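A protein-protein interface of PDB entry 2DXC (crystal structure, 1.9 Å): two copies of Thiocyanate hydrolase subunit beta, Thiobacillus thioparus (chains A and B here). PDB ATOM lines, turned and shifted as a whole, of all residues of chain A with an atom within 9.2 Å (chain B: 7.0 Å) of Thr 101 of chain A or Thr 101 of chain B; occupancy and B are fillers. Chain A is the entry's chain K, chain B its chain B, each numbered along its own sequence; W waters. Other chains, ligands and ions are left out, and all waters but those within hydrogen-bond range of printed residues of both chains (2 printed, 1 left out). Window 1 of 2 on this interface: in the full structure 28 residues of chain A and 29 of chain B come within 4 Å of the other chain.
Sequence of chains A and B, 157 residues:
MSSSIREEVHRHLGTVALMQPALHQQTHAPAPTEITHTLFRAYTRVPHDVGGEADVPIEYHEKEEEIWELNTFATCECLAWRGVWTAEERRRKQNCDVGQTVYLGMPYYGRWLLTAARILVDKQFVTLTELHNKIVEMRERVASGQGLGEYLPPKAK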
ATOM      1  N   THR A  27      21.643  14.303  -2.795  1.00  0.00           N
ATOM      2  CA  THR A  27      20.936  15.454  -3.340  1.00  0.00           C
ATOM      3  C   THR A  27      21.821  16.692  -3.269  1.00  0.00           C
ATOM      4  O   THR A  27      22.277  17.082  -2.192  1.00  0.00           O
ATOM      5  CB  THR A  27      19.628  15.725  -2.573  1.00  0.00           C
ATOM      6  OG1 THR A  27      19.922  15.979  -1.193  1.00  0.00           O
ATOM      7  CG2 THR A  27      18.691  14.529  -2.682  1.00  0.00           C
ATOM      8  N   HIS A  28      22.065  17.304  -4.424  1.00  0.00           N
ATOM      9  CA  HIS A  28      22.900  18.494  -4.496  1.00  0.00           C
ATOM     10  C   HIS A  28      22.148  19.654  -5.133  1.00  0.00           C
ATOM     11  O   HIS A  28      22.364  19.981  -6.301  1.00  0.00           O
ATOM     12  CB  HIS A  28      24.163  18.189  -5.302  1.00  0.00           C
ATOM     13  CG  HIS A  28      24.985  17.073  -4.734  1.00  0.00           C
ATOM     14  ND1 HIS A  28      25.873  17.254  -3.697  1.00  0.00           N
ATOM     15  CD2 HIS A  28      25.036  15.756  -5.048  1.00  0.00           C
ATOM     16  CE1 HIS A  28      26.438  16.098  -3.396  1.00  0.00           C
ATOM     17  NE2 HIS A  28      25.947  15.172  -4.202  1.00  0.00           N
ATOM     18  N   ALA A  29      21.260  20.270  -4.357  1.00  0.00           N
ATOM     19  CA  ALA A  29      20.473  21.403  -4.828  1.00  0.00           C
ATOM     20  C   ALA A  29      19.791  21.122  -6.172  1.00  0.00           C
ATOM     21  O   ALA A  29      20.044  21.803  -7.166  1.00  0.00           O
ATOM     22  CB  ALA A  29      21.369  22.650  -4.933  1.00  0.00           C
ATOM     23  N   PRO A  30      18.907  20.115  -6.215  1.00  0.00           N
ATOM     24  CA  PRO A  30      18.209  19.779  -7.461  1.00  0.00           C
ATOM     25  C   PRO A  30      17.311  20.910  -7.967  1.00  0.00           C
ATOM     26  O   PRO A  30      16.880  21.769  -7.197  1.00  0.00           O
ATOM     27  CB  PRO A  30      17.415  18.529  -7.083  1.00  0.00           C
ATOM     28  CG  PRO A  30      17.140  18.740  -5.622  1.00  0.00           C
ATOM     29  CD  PRO A  30      18.462  19.250  -5.108  1.00  0.00           C
ATOM     30  N   ILE A  35      11.467  18.420  -7.781  1.00  0.00           N
ATOM     31  CA  ILE A  35      10.746  18.410  -6.518  1.00  0.00           C
ATOM     32  C   ILE A  35       9.264  18.179  -6.755  1.00  0.00           C
ATOM     33  O   ILE A  35       8.591  19.014  -7.353  1.00  0.00           O
ATOM     34  CB  ILE A  35      10.920  19.745  -5.765  1.00  0.00           C
ATOM     35  CG1 ILE A  35      12.406  20.026  -5.554  1.00  0.00           C
ATOM     36  CG2 ILE A  35      10.210  19.683  -4.417  1.00  0.00           C
ATOM     37  CD1 ILE A  35      13.133  18.990  -4.673  1.00  0.00           C
ATOM     38  N   LEU A  39       7.769  15.396  -2.168  1.00  0.00           N
ATOM     39  CA  LEU A  39       9.068  15.788  -1.636  1.00  0.00           C
ATOM     40  C   LEU A  39       8.993  17.167  -0.982  1.00  0.00           C
ATOM     41  O   LEU A  39       9.603  17.402   0.059  1.00  0.00           O
ATOM     42  CB  LEU A  39      10.120  15.798  -2.748  1.00  0.00           C
ATOM     43  CG  LEU A  39      10.598  14.433  -3.252  1.00  0.00           C
ATOM     44  CD1 LEU A  39      11.613  14.628  -4.367  1.00  0.00           C
ATOM     45  CD2 LEU A  39      11.221  13.649  -2.101  1.00  0.00           C
ATOM     46  N   ALA A  42       7.639  16.769   2.419  1.00  0.00           N
ATOM     47  CA  ALA A  42       8.600  16.073   3.267  1.00  0.00           C
ATOM     48  C   ALA A  42       9.773  16.980   3.664  1.00  0.00           C
ATOM     49  O   ALA A  42      10.258  16.916   4.793  1.00  0.00           O
ATOM     50  CB  ALA A  42       9.118  14.828   2.554  1.00  0.00           C
ATOM     51  N   TYR A  43      10.228  17.823   2.741  1.00  0.00           N
ATOM     52  CA  TYR A  43      11.338  18.733   3.024  1.00  0.00           C
ATOM     53  C   TYR A  43      10.940  19.905   3.920  1.00  0.00           C
ATOM     54  O   TYR A  43      11.733  20.355   4.752  1.00  0.00           O
ATOM     55  CB  TYR A  43      11.933  19.283   1.719  1.00  0.00           C
ATOM     56  CG  TYR A  43      12.941  18.367   1.050  1.00  0.00           C
ATOM     57  CD1 TYR A  43      14.107  17.978   1.716  1.00  0.00           C
ATOM     58  CD2 TYR A  43      12.723  17.879  -0.241  1.00  0.00           C
ATOM     59  CE1 TYR A  43      15.032  17.117   1.115  1.00  0.00           C
ATOM     60  CE2 TYR A  43      13.642  17.018  -0.852  1.00  0.00           C
ATOM     61  CZ  TYR A  43      14.793  16.640  -0.165  1.00  0.00           C
ATOM     62  OH  TYR A  43      15.692  15.772  -0.748  1.00  0.00           O
ATOM     63  N   THR A  44       9.719  20.403   3.751  1.00  0.00           N
ATOM     64  CA  THR A  44       9.254  21.535   4.544  1.00  0.00           C
ATOM     65  C   THR A  44       8.499  21.111   5.803  1.00  0.00           C
ATOM     66  O   THR A  44       7.904  21.940   6.491  1.00  0.00           O
ATOM     67  CB  THR A  44       8.362  22.477   3.704  1.00  0.00           C
ATOM     68  OG1 THR A  44       7.210  21.769   3.236  1.00  0.00           O
ATOM     69  CG2 THR A  44       9.137  23.006   2.506  1.00  0.00           C
ATOM     70  N   ARG A  45       8.537  19.814   6.093  1.00  0.00           N
ATOM     71  CA  ARG A  45       7.891  19.233   7.270  1.00  0.00           C
ATOM     72  C   ARG A  45       8.475  19.891   8.516  1.00  0.00           C
ATOM     73  O   ARG A  45       9.530  20.520   8.454  1.00  0.00           O
ATOM     74  CB  ARG A  45       8.231  17.741   7.370  1.00  0.00           C
ATOM     75  CG  ARG A  45       9.708  17.546   7.770  1.00  0.00           C
ATOM     76  CD  ARG A  45      10.111  16.113   8.080  1.00  0.00           C
ATOM     77  NE  ARG A  45       9.286  15.525   9.126  1.00  0.00           N
ATOM     78  CZ  ARG A  45       9.587  14.407   9.775  1.00  0.00           C
ATOM     79  NH1 ARG A  45      10.707  13.748   9.496  1.00  0.00           N
ATOM     80  NH2 ARG A  45       8.751  13.933  10.688  1.00  0.00           N
ATOM     81  N   PRO A  47      10.319  19.036  11.649  1.00  0.00           N
ATOM     82  CA  PRO A  47      11.147  17.946  12.181  1.00  0.00           C
ATOM     83  C   PRO A  47      10.653  17.173  13.407  1.00  0.00           C
ATOM     84  O   PRO A  47      10.870  15.963  13.501  1.00  0.00           O
ATOM     85  CB  PRO A  47      12.488  18.631  12.454  1.00  0.00           C
ATOM     86  CG  PRO A  47      12.541  19.685  11.405  1.00  0.00           C
ATOM     87  CD  PRO A  47      11.135  20.244  11.428  1.00  0.00           C
ATOM     88  N   CYS A  96      12.274  22.418  15.891  1.00  0.00           N
ATOM     89  CA  CYS A  96      11.915  22.544  14.488  1.00  0.00           C
ATOM     90  C   CYS A  96      12.924  23.351  13.677  1.00  0.00           C
ATOM     91  O   CYS A  96      13.479  22.846  12.702  1.00  0.00           O
ATOM     92  CB  CYS A  96      10.521  23.164  14.367  1.00  0.00           C
ATOM     93  SG  CYS A  96       9.248  22.269  15.312  1.00  0.00           S
ATOM     94  N   ASP A  97      13.174  24.592  14.090  1.00  0.00           N
ATOM     95  CA  ASP A  97      14.104  25.462  13.372  1.00  0.00           C
ATOM     96  C   ASP A  97      15.502  24.879  13.180  1.00  0.00           C
ATOM     97  O   ASP A  97      16.184  25.240  12.224  1.00  0.00           O
ATOM     98  CB  ASP A  97      14.224  26.826  14.068  1.00  0.00           C
ATOM     99  CG  ASP A  97      12.967  27.678  13.923  1.00  0.00           C
ATOM    100  OD1 ASP A  97      12.011  27.239  13.247  1.00  0.00           O
ATOM    101  OD2 ASP A  97      12.943  28.795  14.491  1.00  0.00           O
ATOM    102  N   VAL A  98      15.937  23.987  14.073  1.00  0.00           N
ATOM    103  CA  VAL A  98      17.277  23.404  13.945  1.00  0.00           C
ATOM    104  C   VAL A  98      17.453  22.587  12.664  1.00  0.00           C
ATOM    105  O   VAL A  98      18.579  22.352  12.218  1.00  0.00           O
ATOM    106  CB  VAL A  98      17.639  22.509  15.161  1.00  0.00           C
ATOM    107  CG1 VAL A  98      17.735  23.363  16.427  1.00  0.00           C
ATOM    108  CG2 VAL A  98      16.601  21.411  15.335  1.00  0.00           C
ATOM    109  N   GLY A  99      16.343  22.155  12.073  1.00  0.00           N
ATOM    110  CA  GLY A  99      16.429  21.390  10.842  1.00  0.00           C
ATOM    111  C   GLY A  99      16.612  19.901  11.054  1.00  0.00           C
ATOM    112  O   GLY A  99      17.116  19.469  12.085  1.00  0.00           O
ATOM    113  N   GLN A 100      16.215  19.124  10.052  1.00  0.00           N
ATOM    114  CA  GLN A 100      16.288  17.663  10.081  1.00  0.00           C
ATOM    115  C   GLN A 100      17.606  17.032  10.555  1.00  0.00           C
ATOM    116  O   GLN A 100      17.602  16.177  11.442  1.00  0.00           O
ATOM    117  CB  GLN A 100      15.942  17.122   8.686  1.00  0.00           C
ATOM    118  CG  GLN A 100      15.809  15.610   8.572  1.00  0.00           C
ATOM    119  CD  GLN A 100      14.676  15.059   9.415  1.00  0.00           C
ATOM    120  OE1 GLN A 100      14.819  14.878  10.627  1.00  0.00           O
ATOM    121  NE2 GLN A 100      13.537  14.802   8.780  1.00  0.00           N
ATOM    122  N   THR A 101      18.729  17.443   9.971  1.00  0.00           N
ATOM    123  CA  THR A 101      20.025  16.857  10.330  1.00  0.00           C
ATOM    124  C   THR A 101      20.428  17.012  11.792  1.00  0.00           C
ATOM    125  O   THR A 101      20.756  16.027  12.457  1.00  0.00           O
ATOM    126  CB  THR A 101      21.157  17.415   9.433  1.00  0.00           C
ATOM    127  OG1 THR A 101      20.928  17.018   8.076  1.00  0.00           O
ATOM    128  CG2 THR A 101      22.517  16.879   9.885  1.00  0.00           C
ATOM    129  N   VAL A 102      20.426  18.242  12.293  1.00  0.00           N
ATOM    130  CA  VAL A 102      20.787  18.486  13.686  1.00  0.00           C
ATOM    131  C   VAL A 102      19.736  17.875  14.618  1.00  0.00           C
ATOM    132  O   VAL A 102      20.060  17.359  15.695  1.00  0.00           O
ATOM    133  CB  VAL A 102      20.898  20.012  13.969  1.00  0.00           C
ATOM    134  CG1 VAL A 102      21.029  20.268  15.467  1.00  0.00           C
ATOM    135  CG2 VAL A 102      22.112  20.591  13.239  1.00  0.00           C
ATOM    136  N   TYR A 103      18.476  17.919  14.195  1.00  0.00           N
ATOM    137  CA  TYR A 103      17.391  17.393  15.012  1.00  0.00           C
ATOM    138  C   TYR A 103      17.607  15.953  15.466  1.00  0.00           C
ATOM    139  O   TYR A 103      17.290  15.600  16.604  1.00  0.00           O
ATOM    140  CB  TYR A 103      16.049  17.484  14.268  1.00  0.00           C
ATOM    141  CG  TYR A 103      14.892  17.073  15.149  1.00  0.00           C
ATOM    142  CD1 TYR A 103      14.600  17.780  16.317  1.00  0.00           C
ATOM    143  CD2 TYR A 103      14.126  15.942  14.854  1.00  0.00           C
ATOM    144  CE1 TYR A 103      13.576  17.370  17.177  1.00  0.00           C
ATOM    145  CE2 TYR A 103      13.101  15.522  15.707  1.00  0.00           C
ATOM    146  CZ  TYR A 103      12.833  16.240  16.866  1.00  0.00           C
ATOM    147  OH  TYR A 103      11.832  15.836  17.721  1.00  0.00           O
ATOM    148  N   LEU A 104      18.141  15.116  14.582  1.00  0.00           N
ATOM    149  CA  LEU A 104      18.366  13.719  14.931  1.00  0.00           C
ATOM    150  C   LEU A 104      19.835  13.328  15.090  1.00  0.00           C
ATOM    151  O   LEU A 104      20.137  12.267  15.635  1.00  0.00           O
ATOM    152  CB  LEU A 104      17.690  12.809  13.899  1.00  0.00           C
ATOM    153  CG  LEU A 104      16.158  12.774  13.998  1.00  0.00           C
ATOM    154  CD1 LEU A 104      15.562  12.035  12.809  1.00  0.00           C
ATOM    155  CD2 LEU A 104      15.758  12.085  15.295  1.00  0.00           C
ATOM    156  N   GLY A 105      20.743  14.184  14.629  1.00  0.00           N
ATOM    157  CA  GLY A 105      22.159  13.883  14.739  1.00  0.00           C
ATOM    158  C   GLY A 105      22.795  14.306  16.053  1.00  0.00           C
ATOM    159  O   GLY A 105      23.774  13.703  16.499  1.00  0.00           O
ATOM    160  N   MET A 106      22.245  15.345  16.676  1.00  0.00           N
ATOM    161  CA  MET A 106      22.777  15.845  17.941  1.00  0.00           C
ATOM    162  C   MET A 106      21.959  15.353  19.130  1.00  0.00           C
ATOM    163  O   MET A 106      20.840  14.862  18.967  1.00  0.00           O
ATOM    164  CB  MET A 106      22.810  17.375  17.918  1.00  0.00           C
ATOM    165  CG  MET A 106      23.913  17.960  17.035  1.00  0.00           C
ATOM    166  SD  MET A 106      25.570  17.795  17.766  1.00  0.00           S
ATOM    167  CE  MET A 106      25.613  19.268  18.797  1.00  0.00           C
ATOM    168  N   PRO A 107      22.511  15.478  20.347  1.00  0.00           N
ATOM    169  CA  PRO A 107      21.793  15.026  21.540  1.00  0.00           C
ATOM    170  C   PRO A 107      20.630  15.939  21.918  1.00  0.00           C
ATOM    171  O   PRO A 107      20.633  17.134  21.621  1.00  0.00           O
ATOM    172  CB  PRO A 107      22.876  15.024  22.627  1.00  0.00           C
ATOM    173  CG  PRO A 107      24.175  15.001  21.858  1.00  0.00           C
ATOM    174  CD  PRO A 107      23.876  15.902  20.700  1.00  0.00           C
ATOM    175  N   ARG A 111      20.544  20.251  21.723  1.00  0.00           N
ATOM    176  CA  ARG A 111      19.645  21.141  20.997  1.00  0.00           C
ATOM    177  C   ARG A 111      19.073  22.206  21.933  1.00  0.00           C
ATOM    178  O   ARG A 111      18.892  23.358  21.535  1.00  0.00           O
ATOM    179  CB  ARG A 111      18.519  20.330  20.345  1.00  0.00           C
ATOM    180  CG  ARG A 111      19.029  19.368  19.264  1.00  0.00           C
ATOM    181  CD  ARG A 111      17.907  18.642  18.510  1.00  0.00           C
ATOM    182  NE  ARG A 111      17.123  17.754  19.366  1.00  0.00           N
ATOM    183  CZ  ARG A 111      15.966  18.083  19.934  1.00  0.00           C
ATOM    184  NH1 ARG A 111      15.444  19.286  19.733  1.00  0.00           N
ATOM    185  NH2 ARG A 111      15.330  17.213  20.706  1.00  0.00           N
ATOM    186  N   THR B  27      21.398   8.028  12.639  1.00  0.00           N
ATOM    187  CA  THR B  27      21.571   8.731  13.905  1.00  0.00           C
ATOM    188  C   THR B  27      20.209   9.115  14.472  1.00  0.00           C
ATOM    189  O   THR B  27      19.454   9.861  13.838  1.00  0.00           O
ATOM    190  CB  THR B  27      22.418  10.010  13.722  1.00  0.00           C
ATOM    191  OG1 THR B  27      21.779  10.874  12.771  1.00  0.00           O
ATOM    192  CG2 THR B  27      23.821   9.660  13.224  1.00  0.00           C
ATOM    193  N   ALA B  42      31.294  19.454  13.013  1.00  0.00           N
ATOM    194  CA  ALA B  42      30.639  19.114  11.755  1.00  0.00           C
ATOM    195  C   ALA B  42      29.134  19.413  11.812  1.00  0.00           C
ATOM    196  O   ALA B  42      28.568  19.952  10.861  1.00  0.00           O
ATOM    197  CB  ALA B  42      30.877  17.633  11.422  1.00  0.00           C
ATOM    198  N   TYR B  43      28.493  19.063  12.925  1.00  0.00           N
ATOM    199  CA  TYR B  43      27.057  19.296  13.090  1.00  0.00           C
ATOM    200  C   TYR B  43      26.690  20.763  13.253  1.00  0.00           C
ATOM    201  O   TYR B  43      25.642  21.196  12.775  1.00  0.00           O
ATOM    202  CB  TYR B  43      26.515  18.518  14.296  1.00  0.00           C
ATOM    203  CG  TYR B  43      26.206  17.069  14.014  1.00  0.00           C
ATOM    204  CD1 TYR B  43      26.824  16.053  14.740  1.00  0.00           C
ATOM    205  CD2 TYR B  43      25.298  16.710  13.015  1.00  0.00           C
ATOM    206  CE1 TYR B  43      26.550  14.715  14.480  1.00  0.00           C
ATOM    207  CE2 TYR B  43      25.016  15.370  12.745  1.00  0.00           C
ATOM    208  CZ  TYR B  43      25.648  14.380  13.480  1.00  0.00           C
ATOM    209  OH  TYR B  43      25.394  13.052  13.208  1.00  0.00           O
ATOM    210  N   PRO B  47      26.177  25.565   7.083  1.00  0.00           N
ATOM    211  CA  PRO B  47      25.903  24.863   5.823  1.00  0.00           C
ATOM    212  C   PRO B  47      26.487  25.397   4.513  1.00  0.00           C
ATOM    213  O   PRO B  47      26.911  24.610   3.664  1.00  0.00           O
ATOM    214  CB  PRO B  47      24.376  24.822   5.781  1.00  0.00           C
ATOM    215  CG  PRO B  47      24.012  24.718   7.221  1.00  0.00           C
ATOM    216  CD  PRO B  47      24.932  25.737   7.856  1.00  0.00           C
ATOM    217  N   VAL B  98      18.569  27.443   7.362  1.00  0.00           N
ATOM    218  CA  VAL B  98      17.713  26.381   6.831  1.00  0.00           C
ATOM    219  C   VAL B  98      18.192  24.984   7.220  1.00  0.00           C
ATOM    220  O   VAL B  98      17.426  24.024   7.168  1.00  0.00           O
ATOM    221  CB  VAL B  98      17.579  26.457   5.284  1.00  0.00           C
ATOM    222  CG1 VAL B  98      16.866  27.742   4.888  1.00  0.00           C
ATOM    223  CG2 VAL B  98      18.948  26.379   4.630  1.00  0.00           C
ATOM    224  N   GLY B  99      19.459  24.870   7.610  1.00  0.00           N
ATOM    225  CA  GLY B  99      19.976  23.575   8.018  1.00  0.00           C
ATOM    226  C   GLY B  99      20.459  22.713   6.866  1.00  0.00           C
ATOM    227  O   GLY B  99      20.012  22.864   5.736  1.00  0.00           O
ATOM    228  N   GLN B 100      21.359  21.788   7.183  1.00  0.00           N
ATOM    229  CA  GLN B 100      21.978  20.886   6.213  1.00  0.00           C
ATOM    230  C   GLN B 100      21.056  20.192   5.209  1.00  0.00           C
ATOM    231  O   GLN B 100      21.287  20.264   4.003  1.00  0.00           O
ATOM    232  CB  GLN B 100      22.790  19.826   6.965  1.00  0.00           C
ATOM    233  CG  GLN B 100      23.652  18.933   6.084  1.00  0.00           C
ATOM    234  CD  GLN B 100      24.761  19.702   5.381  1.00  0.00           C
ATOM    235  OE1 GLN B 100      24.515  20.435   4.421  1.00  0.00           O
ATOM    236  NE2 GLN B 100      25.985  19.548   5.869  1.00  0.00           N
ATOM    237  N   THR B 101      20.022  19.515   5.699  1.00  0.00           N
ATOM    238  CA  THR B 101      19.107  18.790   4.821  1.00  0.00           C
ATOM    239  C   THR B 101      18.409  19.658   3.774  1.00  0.00           C
ATOM    240  O   THR B 101      18.475  19.362   2.578  1.00  0.00           O
ATOM    241  CB  THR B 101      18.049  18.018   5.645  1.00  0.00           C
ATOM    242  OG1 THR B 101      18.706  17.031   6.453  1.00  0.00           O
ATOM    243  CG2 THR B 101      17.051  17.321   4.730  1.00  0.00           C
ATOM    244  N   VAL B 102      17.739  20.720   4.209  1.00  0.00           N
ATOM    245  CA  VAL B 102      17.054  21.595   3.262  1.00  0.00           C
ATOM    246  C   VAL B 102      18.054  22.314   2.355  1.00  0.00           C
ATOM    247  O   VAL B 102      17.798  22.519   1.167  1.00  0.00           O
ATOM    248  CB  VAL B 102      16.192  22.655   3.994  1.00  0.00           C
ATOM    249  CG1 VAL B 102      15.666  23.684   2.998  1.00  0.00           C
ATOM    250  CG2 VAL B 102      15.025  21.973   4.703  1.00  0.00           C
ATOM    251  N   TYR B 103      19.199  22.686   2.920  1.00  0.00           N
ATOM    252  CA  TYR B 103      20.220  23.394   2.160  1.00  0.00           C
ATOM    253  C   TYR B 103      20.609  22.688   0.860  1.00  0.00           C
ATOM    254  O   TYR B 103      20.802  23.339  -0.165  1.00  0.00           O
ATOM    255  CB  TYR B 103      21.477  23.609   3.013  1.00  0.00           C
ATOM    256  CG  TYR B 103      22.504  24.463   2.312  1.00  0.00           C
ATOM    257  CD1 TYR B 103      22.212  25.779   1.961  1.00  0.00           C
ATOM    258  CD2 TYR B 103      23.745  23.941   1.941  1.00  0.00           C
ATOM    259  CE1 TYR B 103      23.125  26.556   1.252  1.00  0.00           C
ATOM    260  CE2 TYR B 103      24.667  24.713   1.227  1.00  0.00           C
ATOM    261  CZ  TYR B 103      24.346  26.016   0.887  1.00  0.00           C
ATOM    262  OH  TYR B 103      25.229  26.780   0.162  1.00  0.00           O
ATOM    263  N   LEU B 104      20.722  21.365   0.894  1.00  0.00           N
ATOM    264  CA  LEU B 104      21.107  20.626  -0.305  1.00  0.00           C
ATOM    265  C   LEU B 104      19.991  19.788  -0.922  1.00  0.00           C
ATOM    266  O   LEU B 104      20.119  19.321  -2.054  1.00  0.00           O
ATOM    267  CB  LEU B 104      22.318  19.736   0.001  1.00  0.00           C
ATOM    268  CG  LEU B 104      23.639  20.486   0.207  1.00  0.00           C
ATOM    269  CD1 LEU B 104      24.677  19.561   0.824  1.00  0.00           C
ATOM    270  CD2 LEU B 104      24.131  21.030  -1.133  1.00  0.00           C
ATOM    271  N   GLY B 105      18.900  19.604  -0.182  1.00  0.00           N
ATOM    272  CA  GLY B 105      17.793  18.808  -0.685  1.00  0.00           C
ATOM    273  C   GLY B 105      16.816  19.595  -1.544  1.00  0.00           C
ATOM    274  O   GLY B 105      16.201  19.050  -2.466  1.00  0.00           O
ATOM    275  N   MET B 106      16.678  20.883  -1.245  1.00  0.00           N
ATOM    276  CA  MET B 106      15.765  21.748  -1.982  1.00  0.00           C
ATOM    277  C   MET B 106      16.485  22.595  -3.027  1.00  0.00           C
ATOM    278  O   MET B 106      17.708  22.716  -3.006  1.00  0.00           O
ATOM    279  CB  MET B 106      15.016  22.653  -1.002  1.00  0.00           C
ATOM    280  CG  MET B 106      13.956  21.928  -0.189  1.00  0.00           C
ATOM    281  SD  MET B 106      12.505  21.511  -1.181  1.00  0.00           S
ATOM    282  CE  MET B 106      11.539  23.029  -0.977  1.00  0.00           C
HETATM  283  O   HOH W   1      25.464  11.774  15.598  1.00  0.00           O
HETATM  284  O   HOH W   2      15.705  16.574  -3.397  1.00  0.00           O
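The backbone carbonyl oxygen of Leu 104 of chain B sits at hydrogen-bond distance from the backbone NH of Ala 29 of chain A (2.7 Å). The backbone carbonyl oxygen of Leu 104 of chain B sits close to the side-chain hydroxyl of Thr 27 of chain A (3.5 Å). The side-chain hydroxyl (OG1) of Thr 101 of chain B sits at hydrogen-bond distance from the side-chain hydroxyl (OG1) of Thr 101 of chain A (2.8 Å). O of Leu 104 of chain A lies close to O of Thr 27 of chain B (3.1 Å).
NE2 of Gln 100 of chain A sits close to NH1 of Arg 45 of chain A, 3.1 Å away.
Of the printed residues of chain B, Thr 101 of chain A touches Gln 100 (3.5 Å) and Thr 101 (2.8 Å). Of chain A, only Gln 100 (3.6 Å) and Thr 101 (2.8 Å) come within 4 Å of Thr 101 of chain B. Of chain A, only Tyr 43 comes within 4 Å of Val 102 of chain B. Of the printed residues of chain B, Leu 104 of chain A touches Thr 27. Of the printed residues of chain B, Ala 29 of chain A touches Leu 104 (2.7 Å) and Met 106 (3.6 Å). Of the printed residues of chain B, His 28 of chain A touches Leu 104. Of the printed residues of chain A, Gly 105 of chain B touches Thr 27, Pro 30, Ile 35 and Tyr 43. Of the printed residues of chain B, Thr 27 of chain A touches Leu 104 and Gly 105. The nearest residue of chain A that does not touch Thr 101 of chain B is Tyr 43 of chain A (4.1 Å).
Thr 27 of chain A touches Gly 105 of chain B, and with the chains exchanged Gly 105 of chain A touches Thr 27 of chain B. Tyr 43 of chain A touches Val 102 of chain B, and with the chains exchanged Val 102 of chain A touches Tyr 43 of chain B. Tyr 43 of chain A touches Gly 105 of chain B, and with the chains exchanged Gly 105 of chain A touches Tyr 43 of chain B. Gln 100 of chain A touches Thr 101 of chain B, and with the chains exchanged Thr 101 of chain A touches Gln 100 of chain B. Of the 19 pairs that touch across the chains among the printed residues, 13 have their exchanged pair printed and touching as well.
Water W2 lies within hydrogen-bond range of O of Gly 105 of chain B (2.7 Å) and OH of Tyr 43 of chain A (2.8 Å). Water W1 lies within hydrogen-bond range of the side-chain hydroxyl (OH) of Tyr 43 of chain B (2.7 Å) and the backbone carbonyl oxygen (O) of Gly 105 of chain A (2.7 Å).
OG1 of Thr 27 of chain A touches CA of Gly 105 of chain B, 3.6 Å away. Leu 104 of chain B touches Pro 30 of chain A (O to CD, 3.5 Å). Pro 30 of chain A touches Gly 105 of chain B. CD1 of Ile 35 of chain A touches O of Gly 105 of chain B, 3.8 Å away. Tyr 43 of chain A touches Gly 105 of chain B (CZ to O, 3.6 Å). CB of Gln 100 of chain A touches OG1 of Thr 101 of chain B, 3.6 Å away. CB of Gln 100 of chain B touches OG1 of Thr 101 of chain A, at 3.5 Å. Val 102 of chain A touches Tyr 43 of chain B. CA of Gly 105 of chain A touches OG1 of Thr 27 of chain B, at 3.6 Å. Met 106 of chain A touches Tyr 43 of chain B (SD to CB, 3.7 Å).
Of the 24 printed residues of chain A, 12 touch a printed residue of chain B. Hydrophobic or aromatic side chains of chain A within 4 Å of the printed part of chain B: Pro 30, Ile 35, Tyr 43, Val 102, Leu 104 and Met 106. Printed residues of chain B that touch a printed residue of chain A: Thr 27, Tyr 43, Gln 100, Thr 101, Val 102, Leu 104, Gly 105 and Met 106. Among the printed residues, 19 pairs touch across the chains.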
